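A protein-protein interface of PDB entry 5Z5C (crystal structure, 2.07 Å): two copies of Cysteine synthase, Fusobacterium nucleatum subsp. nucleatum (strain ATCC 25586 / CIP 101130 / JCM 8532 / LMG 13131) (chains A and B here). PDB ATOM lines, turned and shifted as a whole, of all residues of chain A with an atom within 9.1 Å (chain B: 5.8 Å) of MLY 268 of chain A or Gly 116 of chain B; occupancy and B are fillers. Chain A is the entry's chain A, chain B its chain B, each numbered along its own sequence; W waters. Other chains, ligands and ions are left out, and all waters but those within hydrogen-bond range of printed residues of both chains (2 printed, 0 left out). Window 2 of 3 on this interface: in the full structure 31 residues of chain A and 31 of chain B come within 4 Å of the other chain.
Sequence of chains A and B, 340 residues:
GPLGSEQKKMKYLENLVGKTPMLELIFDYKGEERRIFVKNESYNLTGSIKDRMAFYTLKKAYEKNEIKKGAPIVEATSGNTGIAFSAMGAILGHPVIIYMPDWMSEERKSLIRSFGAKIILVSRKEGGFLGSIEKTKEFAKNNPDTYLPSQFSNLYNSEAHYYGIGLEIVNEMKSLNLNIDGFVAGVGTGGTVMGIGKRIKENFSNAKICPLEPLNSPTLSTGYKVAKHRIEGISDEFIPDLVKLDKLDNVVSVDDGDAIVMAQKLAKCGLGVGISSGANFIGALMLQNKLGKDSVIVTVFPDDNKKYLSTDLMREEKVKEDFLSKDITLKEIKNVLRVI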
ATOM      1  N   VAL A 261      28.065  16.974  23.694  1.00  0.00           N
ATOM      2  CA  VAL A 261      28.255  18.351  23.323  1.00  0.00           C
ATOM      3  C   VAL A 261      29.105  18.379  22.043  1.00  0.00           C
ATOM      4  O   VAL A 261      28.757  19.079  21.109  1.00  0.00           O
ATOM      5  CB  VAL A 261      28.902  19.249  24.431  1.00  0.00           C
ATOM      6  CG1 VAL A 261      29.176  20.663  23.864  1.00  0.00           C
ATOM      7  CG2 VAL A 261      27.971  19.343  25.650  1.00  0.00           C
ATOM      8  N   MET A 262      30.181  17.596  21.981  1.00  0.00           N
ATOM      9  CA  MET A 262      30.972  17.544  20.740  1.00  0.00           C
ATOM     10  C   MET A 262      30.170  17.092  19.493  1.00  0.00           C
ATOM     11  O   MET A 262      30.324  17.662  18.398  1.00  0.00           O
ATOM     12  CB  MET A 262      32.234  16.706  20.908  1.00  0.00           C
ATOM     13  CG  MET A 262      33.241  16.889  19.774  1.00  0.00           C
ATOM     14  SD  MET A 262      33.832  18.598  19.836  1.00  0.00           S
ATOM     15  CE  MET A 262      33.497  19.148  18.164  1.00  0.00           C
ATOM     16  N   ALA A 263      29.286  16.109  19.651  1.00  0.00           N
ATOM     17  CA  ALA A 263      28.477  15.632  18.511  1.00  0.00           C
ATOM     18  C   ALA A 263      27.490  16.755  18.061  1.00  0.00           C
ATOM     19  O   ALA A 263      27.208  16.956  16.839  1.00  0.00           O
ATOM     20  CB  ALA A 263      27.720  14.358  18.876  1.00  0.00           C
ATOM     21  N   GLN A 264      26.977  17.490  19.057  1.00  0.00           N
ATOM     22  CA  GLN A 264      26.107  18.648  18.773  1.00  0.00           C
ATOM     23  C   GLN A 264      26.844  19.735  17.975  1.00  0.00           C
ATOM     24  O   GLN A 264      26.306  20.257  16.972  1.00  0.00           O
ATOM     25  CB  GLN A 264      25.549  19.211  20.069  1.00  0.00           C
ATOM     26  CG  GLN A 264      24.540  18.310  20.749  1.00  0.00           C
ATOM     27  CD  GLN A 264      24.150  18.810  22.127  1.00  0.00           C
ATOM     28  OE1 GLN A 264      24.867  19.576  22.759  1.00  0.00           O
ATOM     29  NE2 GLN A 264      23.019  18.340  22.608  1.00  0.00           N
ATOM     30  N   MLY A 265      28.082  20.028  18.344  1.00  0.00           N
ATOM     31  CA  MLY A 265      28.901  21.006  17.580  1.00  0.00           C
ATOM     32  CB  MLY A 265      30.260  21.191  18.232  1.00  0.00           C
ATOM     33  CG  MLY A 265      30.147  22.107  19.434  1.00  0.00           C
ATOM     34  CD  MLY A 265      31.514  22.395  20.051  1.00  0.00           C
ATOM     35  CE  MLY A 265      31.357  22.796  21.517  1.00  0.00           C
ATOM     36  NZ  MLY A 265      31.478  24.249  21.737  1.00  0.00           N
ATOM     37  CH1 MLY A 265      30.693  25.036  20.771  1.00  0.00           C
ATOM     38  CH2 MLY A 265      31.001  24.550  23.097  1.00  0.00           C
ATOM     39  C   MLY A 265      29.117  20.555  16.169  1.00  0.00           C
ATOM     40  O   MLY A 265      28.997  21.357  15.234  1.00  0.00           O
ATOM     41  N   LEU A 266      29.491  19.281  15.997  1.00  0.00           N
ATOM     42  CA  LEU A 266      29.704  18.712  14.674  1.00  0.00           C
ATOM     43  C   LEU A 266      28.508  18.849  13.728  1.00  0.00           C
ATOM     44  O   LEU A 266      28.684  19.211  12.530  1.00  0.00           O
ATOM     45  CB  LEU A 266      30.138  17.237  14.789  1.00  0.00           C
ATOM     46  CG  LEU A 266      31.582  17.094  15.233  1.00  0.00           C
ATOM     47  CD1 LEU A 266      31.842  15.697  15.797  1.00  0.00           C
ATOM     48  CD2 LEU A 266      32.543  17.440  14.089  1.00  0.00           C
ATOM     49  N   ALA A 267      27.303  18.640  14.256  1.00  0.00           N
ATOM     50  CA  ALA A 267      26.054  18.775  13.467  1.00  0.00           C
ATOM     51  C   ALA A 267      25.802  20.243  13.041  1.00  0.00           C
ATOM     52  O   ALA A 267      25.466  20.519  11.860  1.00  0.00           O
ATOM     53  CB  ALA A 267      24.858  18.227  14.248  1.00  0.00           C
ATOM     54  N   MLY A 268      26.024  21.161  13.979  1.00  0.00           N
ATOM     55  CA  MLY A 268      25.992  22.639  13.699  1.00  0.00           C
ATOM     56  CB  MLY A 268      26.290  23.432  14.967  1.00  0.00           C
ATOM     57  CG  MLY A 268      25.019  23.814  15.711  1.00  0.00           C
ATOM     58  CD  MLY A 268      25.366  24.478  17.041  1.00  0.00           C
ATOM     59  CE  MLY A 268      24.345  25.540  17.420  1.00  0.00           C
ATOM     60  NZ  MLY A 268      23.006  24.931  17.472  1.00  0.00           N
ATOM     61  C   MLY A 268      27.005  23.012  12.648  1.00  0.00           C
ATOM     62  O   MLY A 268      26.881  24.077  12.065  1.00  0.00           O
ATOM     63  N   CYS A 269      28.042  22.211  12.394  1.00  0.00           N
ATOM     64  CA  CYS A 269      28.980  22.531  11.307  1.00  0.00           C
ATOM     65  C   CYS A 269      28.716  21.675  10.048  1.00  0.00           C
ATOM     66  O   CYS A 269      29.476  21.716   9.087  1.00  0.00           O
ATOM     67  CB  CYS A 269      30.442  22.477  11.802  1.00  0.00           C
ATOM     68  SG  CYS A 269      31.269  20.918  11.422  1.00  0.00           S
ATOM     69  N   GLY A 270      27.601  20.945  10.022  1.00  0.00           N
ATOM     70  CA  GLY A 270      27.173  20.234   8.820  1.00  0.00           C
ATOM     71  C   GLY A 270      27.320  18.712   8.872  1.00  0.00           C
ATOM     72  O   GLY A 270      26.948  18.040   7.915  1.00  0.00           O
ATOM     73  N   LEU A 271      27.860  18.201   9.981  1.00  0.00           N
ATOM     74  CA  LEU A 271      28.253  16.806  10.134  1.00  0.00           C
ATOM     75  C   LEU A 271      27.379  16.217  11.202  1.00  0.00           C
ATOM     76  O   LEU A 271      27.693  16.267  12.377  1.00  0.00           O
ATOM     77  CB  LEU A 271      29.725  16.712  10.502  1.00  0.00           C
ATOM     78  CG  LEU A 271      30.624  17.291   9.437  1.00  0.00           C
ATOM     79  CD1 LEU A 271      32.061  17.315   9.904  1.00  0.00           C
ATOM     80  CD2 LEU A 271      30.486  16.523   8.134  1.00  0.00           C
ATOM     81  N   GLY A 272      26.244  15.702  10.756  1.00  0.00           N
ATOM     82  CA  GLY A 272      25.286  15.094  11.640  1.00  0.00           C
ATOM     83  C   GLY A 272      25.739  13.695  12.023  1.00  0.00           C
ATOM     84  O   GLY A 272      25.536  12.747  11.245  1.00  0.00           O
ATOM     85  N   VAL A 273      26.280  13.559  13.218  1.00  0.00           N
ATOM     86  CA  VAL A 273      26.928  12.301  13.657  1.00  0.00           C
ATOM     87  C   VAL A 273      26.379  11.769  14.977  1.00  0.00           C
ATOM     88  O   VAL A 273      25.742  12.500  15.697  1.00  0.00           O
ATOM     89  CB  VAL A 273      28.423  12.514  13.789  1.00  0.00           C
ATOM     90  CG1 VAL A 273      29.011  12.918  12.444  1.00  0.00           C
ATOM     91  CG2 VAL A 273      28.749  13.558  14.881  1.00  0.00           C
ATOM     92  N   ASN A 305      23.341  11.217  12.950  1.00  0.00           N
ATOM     93  CA  ASN A 305      22.567  11.640  14.125  1.00  0.00           C
ATOM     94  C   ASN A 305      21.100  11.134  14.116  1.00  0.00           C
ATOM     95  O   ASN A 305      20.410  11.337  15.114  1.00  0.00           O
ATOM     96  CB  ASN A 305      22.680  13.188  14.367  1.00  0.00           C
ATOM     97  CG  ASN A 305      22.188  14.025  13.196  1.00  0.00           C
ATOM     98  OD1 ASN A 305      21.955  13.528  12.060  1.00  0.00           O
ATOM     99  ND2 ASN A 305      22.000  15.305  13.464  1.00  0.00           N
ATOM    100  N   LEU A 313      21.298  13.508  23.000  1.00  0.00           N
ATOM    101  CA  LEU A 313      21.892  14.290  21.907  1.00  0.00           C
ATOM    102  C   LEU A 313      21.043  15.506  21.472  1.00  0.00           C
ATOM    103  O   LEU A 313      21.571  16.560  21.107  1.00  0.00           O
ATOM    104  CB  LEU A 313      22.150  13.396  20.680  1.00  0.00           C
ATOM    105  CG  LEU A 313      22.853  14.069  19.487  1.00  0.00           C
ATOM    106  CD1 LEU A 313      24.257  14.578  19.887  1.00  0.00           C
ATOM    107  CD2 LEU A 313      22.893  13.115  18.301  1.00  0.00           C
ATOM    108  N   MET A 314      19.730  15.342  21.523  1.00  0.00           N
ATOM    109  CA  MET A 314      18.786  16.410  21.177  1.00  0.00           C
ATOM    110  C   MET A 314      18.365  17.284  22.353  1.00  0.00           C
ATOM    111  O   MET A 314      17.467  18.085  22.203  1.00  0.00           O
ATOM    112  CB  MET A 314      17.527  15.788  20.536  1.00  0.00           C
ATOM    113  CG  MET A 314      17.656  15.429  19.080  1.00  0.00           C
ATOM    114  SD  MET A 314      19.286  15.089  18.370  1.00  0.00           S
ATOM    115  CE  MET A 314      19.648  16.681  17.636  1.00  0.00           C
ATOM    116  N   LEU A 330      34.762  24.678  16.200  1.00  0.00           N
ATOM    117  CA  LEU A 330      34.955  24.119  14.883  1.00  0.00           C
ATOM    118  C   LEU A 330      35.153  25.248  13.875  1.00  0.00           C
ATOM    119  O   LEU A 330      34.414  26.231  13.922  1.00  0.00           O
ATOM    120  CB  LEU A 330      33.726  23.290  14.498  1.00  0.00           C
ATOM    121  CG  LEU A 330      33.569  21.995  15.293  1.00  0.00           C
ATOM    122  CD1 LEU A 330      32.246  21.306  14.939  1.00  0.00           C
ATOM    123  CD2 LEU A 330      34.764  21.083  15.035  1.00  0.00           C
ATOM    124  N   MLY A 331      36.136  25.118  12.987  1.00  0.00           N
ATOM    125  CA  MLY A 331      36.424  26.204  12.024  1.00  0.00           C
ATOM    126  CB  MLY A 331      37.925  26.493  11.950  1.00  0.00           C
ATOM    127  CG  MLY A 331      38.394  27.328  13.142  1.00  0.00           C
ATOM    128  CD  MLY A 331      39.248  28.529  12.709  1.00  0.00           C
ATOM    129  CE  MLY A 331      38.737  29.843  13.304  1.00  0.00           C
ATOM    130  NZ  MLY A 331      39.753  30.428  14.194  1.00  0.00           N
ATOM    131  C   MLY A 331      35.899  25.830  10.674  1.00  0.00           C
ATOM    132  O   MLY A 331      35.049  26.553  10.134  1.00  0.00           O
ATOM    133  N   ILE A 333      35.866  22.499   7.224  1.00  0.00           N
ATOM    134  CA  ILE A 333      36.320  21.324   6.521  1.00  0.00           C
ATOM    135  C   ILE A 333      37.314  21.791   5.476  1.00  0.00           C
ATOM    136  O   ILE A 333      36.950  22.471   4.520  1.00  0.00           O
ATOM    137  CB  ILE A 333      35.135  20.576   5.909  1.00  0.00           C
ATOM    138  CG1 ILE A 333      34.208  20.094   7.038  1.00  0.00           C
ATOM    139  CG2 ILE A 333      35.606  19.448   5.041  1.00  0.00           C
ATOM    140  CD1 ILE A 333      32.819  19.770   6.565  1.00  0.00           C
ATOM    141  N   SER B  86      20.642  23.352   5.173  1.00  0.00           N
ATOM    142  CA  SER B  86      21.137  23.626   6.526  1.00  0.00           C
ATOM    143  C   SER B  86      22.588  23.123   6.692  1.00  0.00           C
ATOM    144  O   SER B  86      23.494  23.886   7.088  1.00  0.00           O
ATOM    145  CB  SER B  86      20.237  23.038   7.593  1.00  0.00           C
ATOM    146  OG  SER B  86      18.948  23.622   7.537  1.00  0.00           O
ATOM    147  N   ALA B  90      25.979  25.519   6.415  1.00  0.00           N
ATOM    148  CA  ALA B  90      26.857  25.605   7.553  1.00  0.00           C
ATOM    149  C   ALA B  90      28.290  25.279   7.136  1.00  0.00           C
ATOM    150  O   ALA B  90      29.197  25.964   7.518  1.00  0.00           O
ATOM    151  CB  ALA B  90      26.364  24.678   8.632  1.00  0.00           C
ATOM    152  N   VAL B  96      21.548  29.852   8.164  1.00  0.00           N
ATOM    153  CA  VAL B  96      20.464  29.308   7.351  1.00  0.00           C
ATOM    154  C   VAL B  96      19.176  29.557   8.121  1.00  0.00           C
ATOM    155  O   VAL B  96      19.110  29.356   9.363  1.00  0.00           O
ATOM    156  CB  VAL B  96      20.634  27.795   7.019  1.00  0.00           C
ATOM    157  CG1 VAL B  96      19.456  27.277   6.216  1.00  0.00           C
ATOM    158  CG2 VAL B  96      21.923  27.577   6.235  1.00  0.00           C
ATOM    159  N   ILE B 112      16.403  19.466  11.670  1.00  0.00           N
ATOM    160  CA  ILE B 112      16.857  20.678  10.966  1.00  0.00           C
ATOM    161  C   ILE B 112      17.578  21.583  11.927  1.00  0.00           C
ATOM    162  O   ILE B 112      18.606  22.141  11.546  1.00  0.00           O
ATOM    163  CB  ILE B 112      15.693  21.407  10.233  1.00  0.00           C
ATOM    164  CG1 ILE B 112      15.291  20.619   9.003  1.00  0.00           C
ATOM    165  CG2 ILE B 112      16.097  22.819   9.831  1.00  0.00           C
ATOM    166  CD1 ILE B 112      13.959  21.029   8.414  1.00  0.00           C
ATOM    167  N   ARG B 113      17.062  21.700  13.162  1.00  0.00           N
ATOM    168  CA  ARG B 113      17.724  22.496  14.216  1.00  0.00           C
ATOM    169  C   ARG B 113      19.101  21.975  14.540  1.00  0.00           C
ATOM    170  O   ARG B 113      19.956  22.786  14.906  1.00  0.00           O
ATOM    171  CB  ARG B 113      16.920  22.605  15.537  1.00  0.00           C
ATOM    172  CG  ARG B 113      15.999  23.811  15.596  1.00  0.00           C
ATOM    173  CD  ARG B 113      15.369  23.994  16.976  1.00  0.00           C
ATOM    174  NE  ARG B 113      14.402  22.941  17.285  1.00  0.00           N
ATOM    175  CZ  ARG B 113      14.651  21.893  18.084  1.00  0.00           C
ATOM    176  NH1 ARG B 113      15.831  21.774  18.690  1.00  0.00           N
ATOM    177  NH2 ARG B 113      13.710  20.977  18.290  1.00  0.00           N
ATOM    178  N   SER B 114      19.316  20.642  14.399  1.00  0.00           N
ATOM    179  CA  SER B 114      20.617  20.035  14.730  1.00  0.00           C
ATOM    180  C   SER B 114      21.708  20.597  13.863  1.00  0.00           C
ATOM    181  O   SER B 114      22.838  20.737  14.303  1.00  0.00           O
ATOM    182  CB  SER B 114      20.619  18.492  14.619  1.00  0.00           C
ATOM    183  OG  SER B 114      20.663  18.022  13.277  1.00  0.00           O
ATOM    184  N   PHE B 115      21.353  20.933  12.634  1.00  0.00           N
ATOM    185  CA  PHE B 115      22.317  21.392  11.645  1.00  0.00           C
ATOM    186  C   PHE B 115      22.561  22.931  11.675  1.00  0.00           C
ATOM    187  O   PHE B 115      23.101  23.488  10.728  1.00  0.00           O
ATOM    188  CB  PHE B 115      21.864  20.924  10.263  1.00  0.00           C
ATOM    189  CG  PHE B 115      22.105  19.472   9.996  1.00  0.00           C
ATOM    190  CD1 PHE B 115      23.388  18.999   9.752  1.00  0.00           C
ATOM    191  CD2 PHE B 115      21.051  18.573   9.968  1.00  0.00           C
ATOM    192  CE1 PHE B 115      23.603  17.656   9.457  1.00  0.00           C
ATOM    193  CE2 PHE B 115      21.266  17.236   9.684  1.00  0.00           C
ATOM    194  CZ  PHE B 115      22.548  16.775   9.439  1.00  0.00           C
ATOM    195  N   GLY B 116      22.140  23.595  12.750  1.00  0.00           N
ATOM    196  CA  GLY B 116      22.461  24.985  13.007  1.00  0.00           C
ATOM    197  C   GLY B 116      21.494  25.980  12.383  1.00  0.00           C
ATOM    198  O   GLY B 116      21.704  27.155  12.518  1.00  0.00           O
ATOM    199  N   ALA B 117      20.431  25.543  11.716  1.00  0.00           N
ATOM    200  CA  ALA B 117      19.532  26.513  11.084  1.00  0.00           C
ATOM    201  C   ALA B 117      18.585  27.186  12.083  1.00  0.00           C
ATOM    202  O   ALA B 117      18.206  26.619  13.114  1.00  0.00           O
ATOM    203  CB  ALA B 117      18.748  25.891   9.956  1.00  0.00           C
ATOM    204  N   MLY B 118      18.180  28.395  11.733  1.00  0.00           N
ATOM    205  CA  MLY B 118      17.199  29.113  12.510  1.00  0.00           C
ATOM    206  CB  MLY B 118      17.463  30.617  12.426  1.00  0.00           C
ATOM    207  CG  MLY B 118      18.946  30.939  12.649  1.00  0.00           C
ATOM    208  CD  MLY B 118      19.222  31.416  14.075  1.00  0.00           C
ATOM    209  CE  MLY B 118      19.891  30.323  14.906  1.00  0.00           C
ATOM    210  NZ  MLY B 118      19.931  30.739  16.315  1.00  0.00           N
ATOM    211  C   MLY B 118      15.842  28.788  11.965  1.00  0.00           C
ATOM    212  O   MLY B 118      15.633  28.915  10.780  1.00  0.00           O
HETATM  213  O   HOH W   1      16.167  19.069  19.336  1.00  0.00           O
HETATM  214  O   HOH W   2      23.756  20.444  16.689  1.00  0.00           O
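The backbone carbonyl oxygen (O) of Ser 114 of chain B lies within hydrogen-bond range of N of MLY 268 of chain A. The side-chain amide nitrogen of Asn 305 of chain A sits at hydrogen-bond distance from the side-chain hydroxyl of Ser 114 of chain B, at 3.0 Å.
Of the printed residues of chain B, MLY 268 of chain A touches Ala 90, Ser 114, Phe 115 and Gly 116. Printed residues of chain A within 4 Å of Gly 116 of chain B: MLY 268 (3.9 Å). Printed residues of chain A within 4 Å of Ser 114 of chain B: Ala 267 (3.2 Å), MLY 268 (3.2 Å), Asn 305 (3.0 Å) and Met 314 (3.7 Å). Of the printed residues of chain A, Ala 90 of chain B touches MLY 268 (3.5 Å). Printed residues of chain B within 4 Å of Asn 305 of chain A: Ser 114 (3.0 Å). Printed residues of chain B within 4 Å of Gly 270 of chain A: Phe 115 (3.7 Å). Ile 112 of chain B touches none of the printed residues of chain A. The nearest printed residue of chain B that does not touch MLY 268 of chain A is Arg 113 of chain B (4.5 Å). The nearest printed residue of chain A that does not touch Ser 114 of chain B is Gln 264 of chain A (4.4 Å).
No position is printed for both chains. Of the 10 pairs that touch across the chains among the printed residues, none has its exchanged pair printed and touching as well.
O of Gly 272 of chain A sits at hydrogen-bond distance from N of Asn 305 of chain A (3.2 Å).
Among the printed residues, pairs that only touch across the chains: Ala 267 of chain A with Ser 114 of chain B, Ala 267 of chain A with Phe 115 of chain B, MLY 268 of chain A with Ala 90 of chain B, Gly 272 of chain A with Phe 115 of chain B, Met 314 of chain A with Ser 114 of chain B, Gly 270 of chain A with Phe 115 of chain B, MLY 268 of chain A with Gly 116 of chain B and MLY 268 of chain A with Phe 115 of chain B.
Water W2 lies within hydrogen-bond range of O of Gln 264 of chain A (2.6 Å) and O of Ser 114 of chain B (2.6 Å). Water W1 lies within hydrogen-bond range of NH1 of Arg 113 of chain B (2.8 Å) and O of Met 314 of chain A (3.3 Å).
Of the 10 printed residues of chain B, 4 touch a printed residue of chain A. Hydrophobic or aromatic side chains of chain B within 4 Å of the printed part of chain A: Ala 90 and Phe 115. Of the 19 printed residues of chain A, 6 touch a printed residue of chain B. Printed residues of chain A that touch a printed residue of chain B: Ala 267, MLY 268, Gly 270, Gly 272, Asn 305 and Met 314. Hydrophobic or aromatic side chains of chain A that line the printed part of chain B: Ala 267 and Met 314. Among the printed residues, 10 pairs touch across the chains. Among the printed residues, no Asp or Glu carboxylate lies within 4 Å of a Lys or Arg side-chain nitrogen of the other chain.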
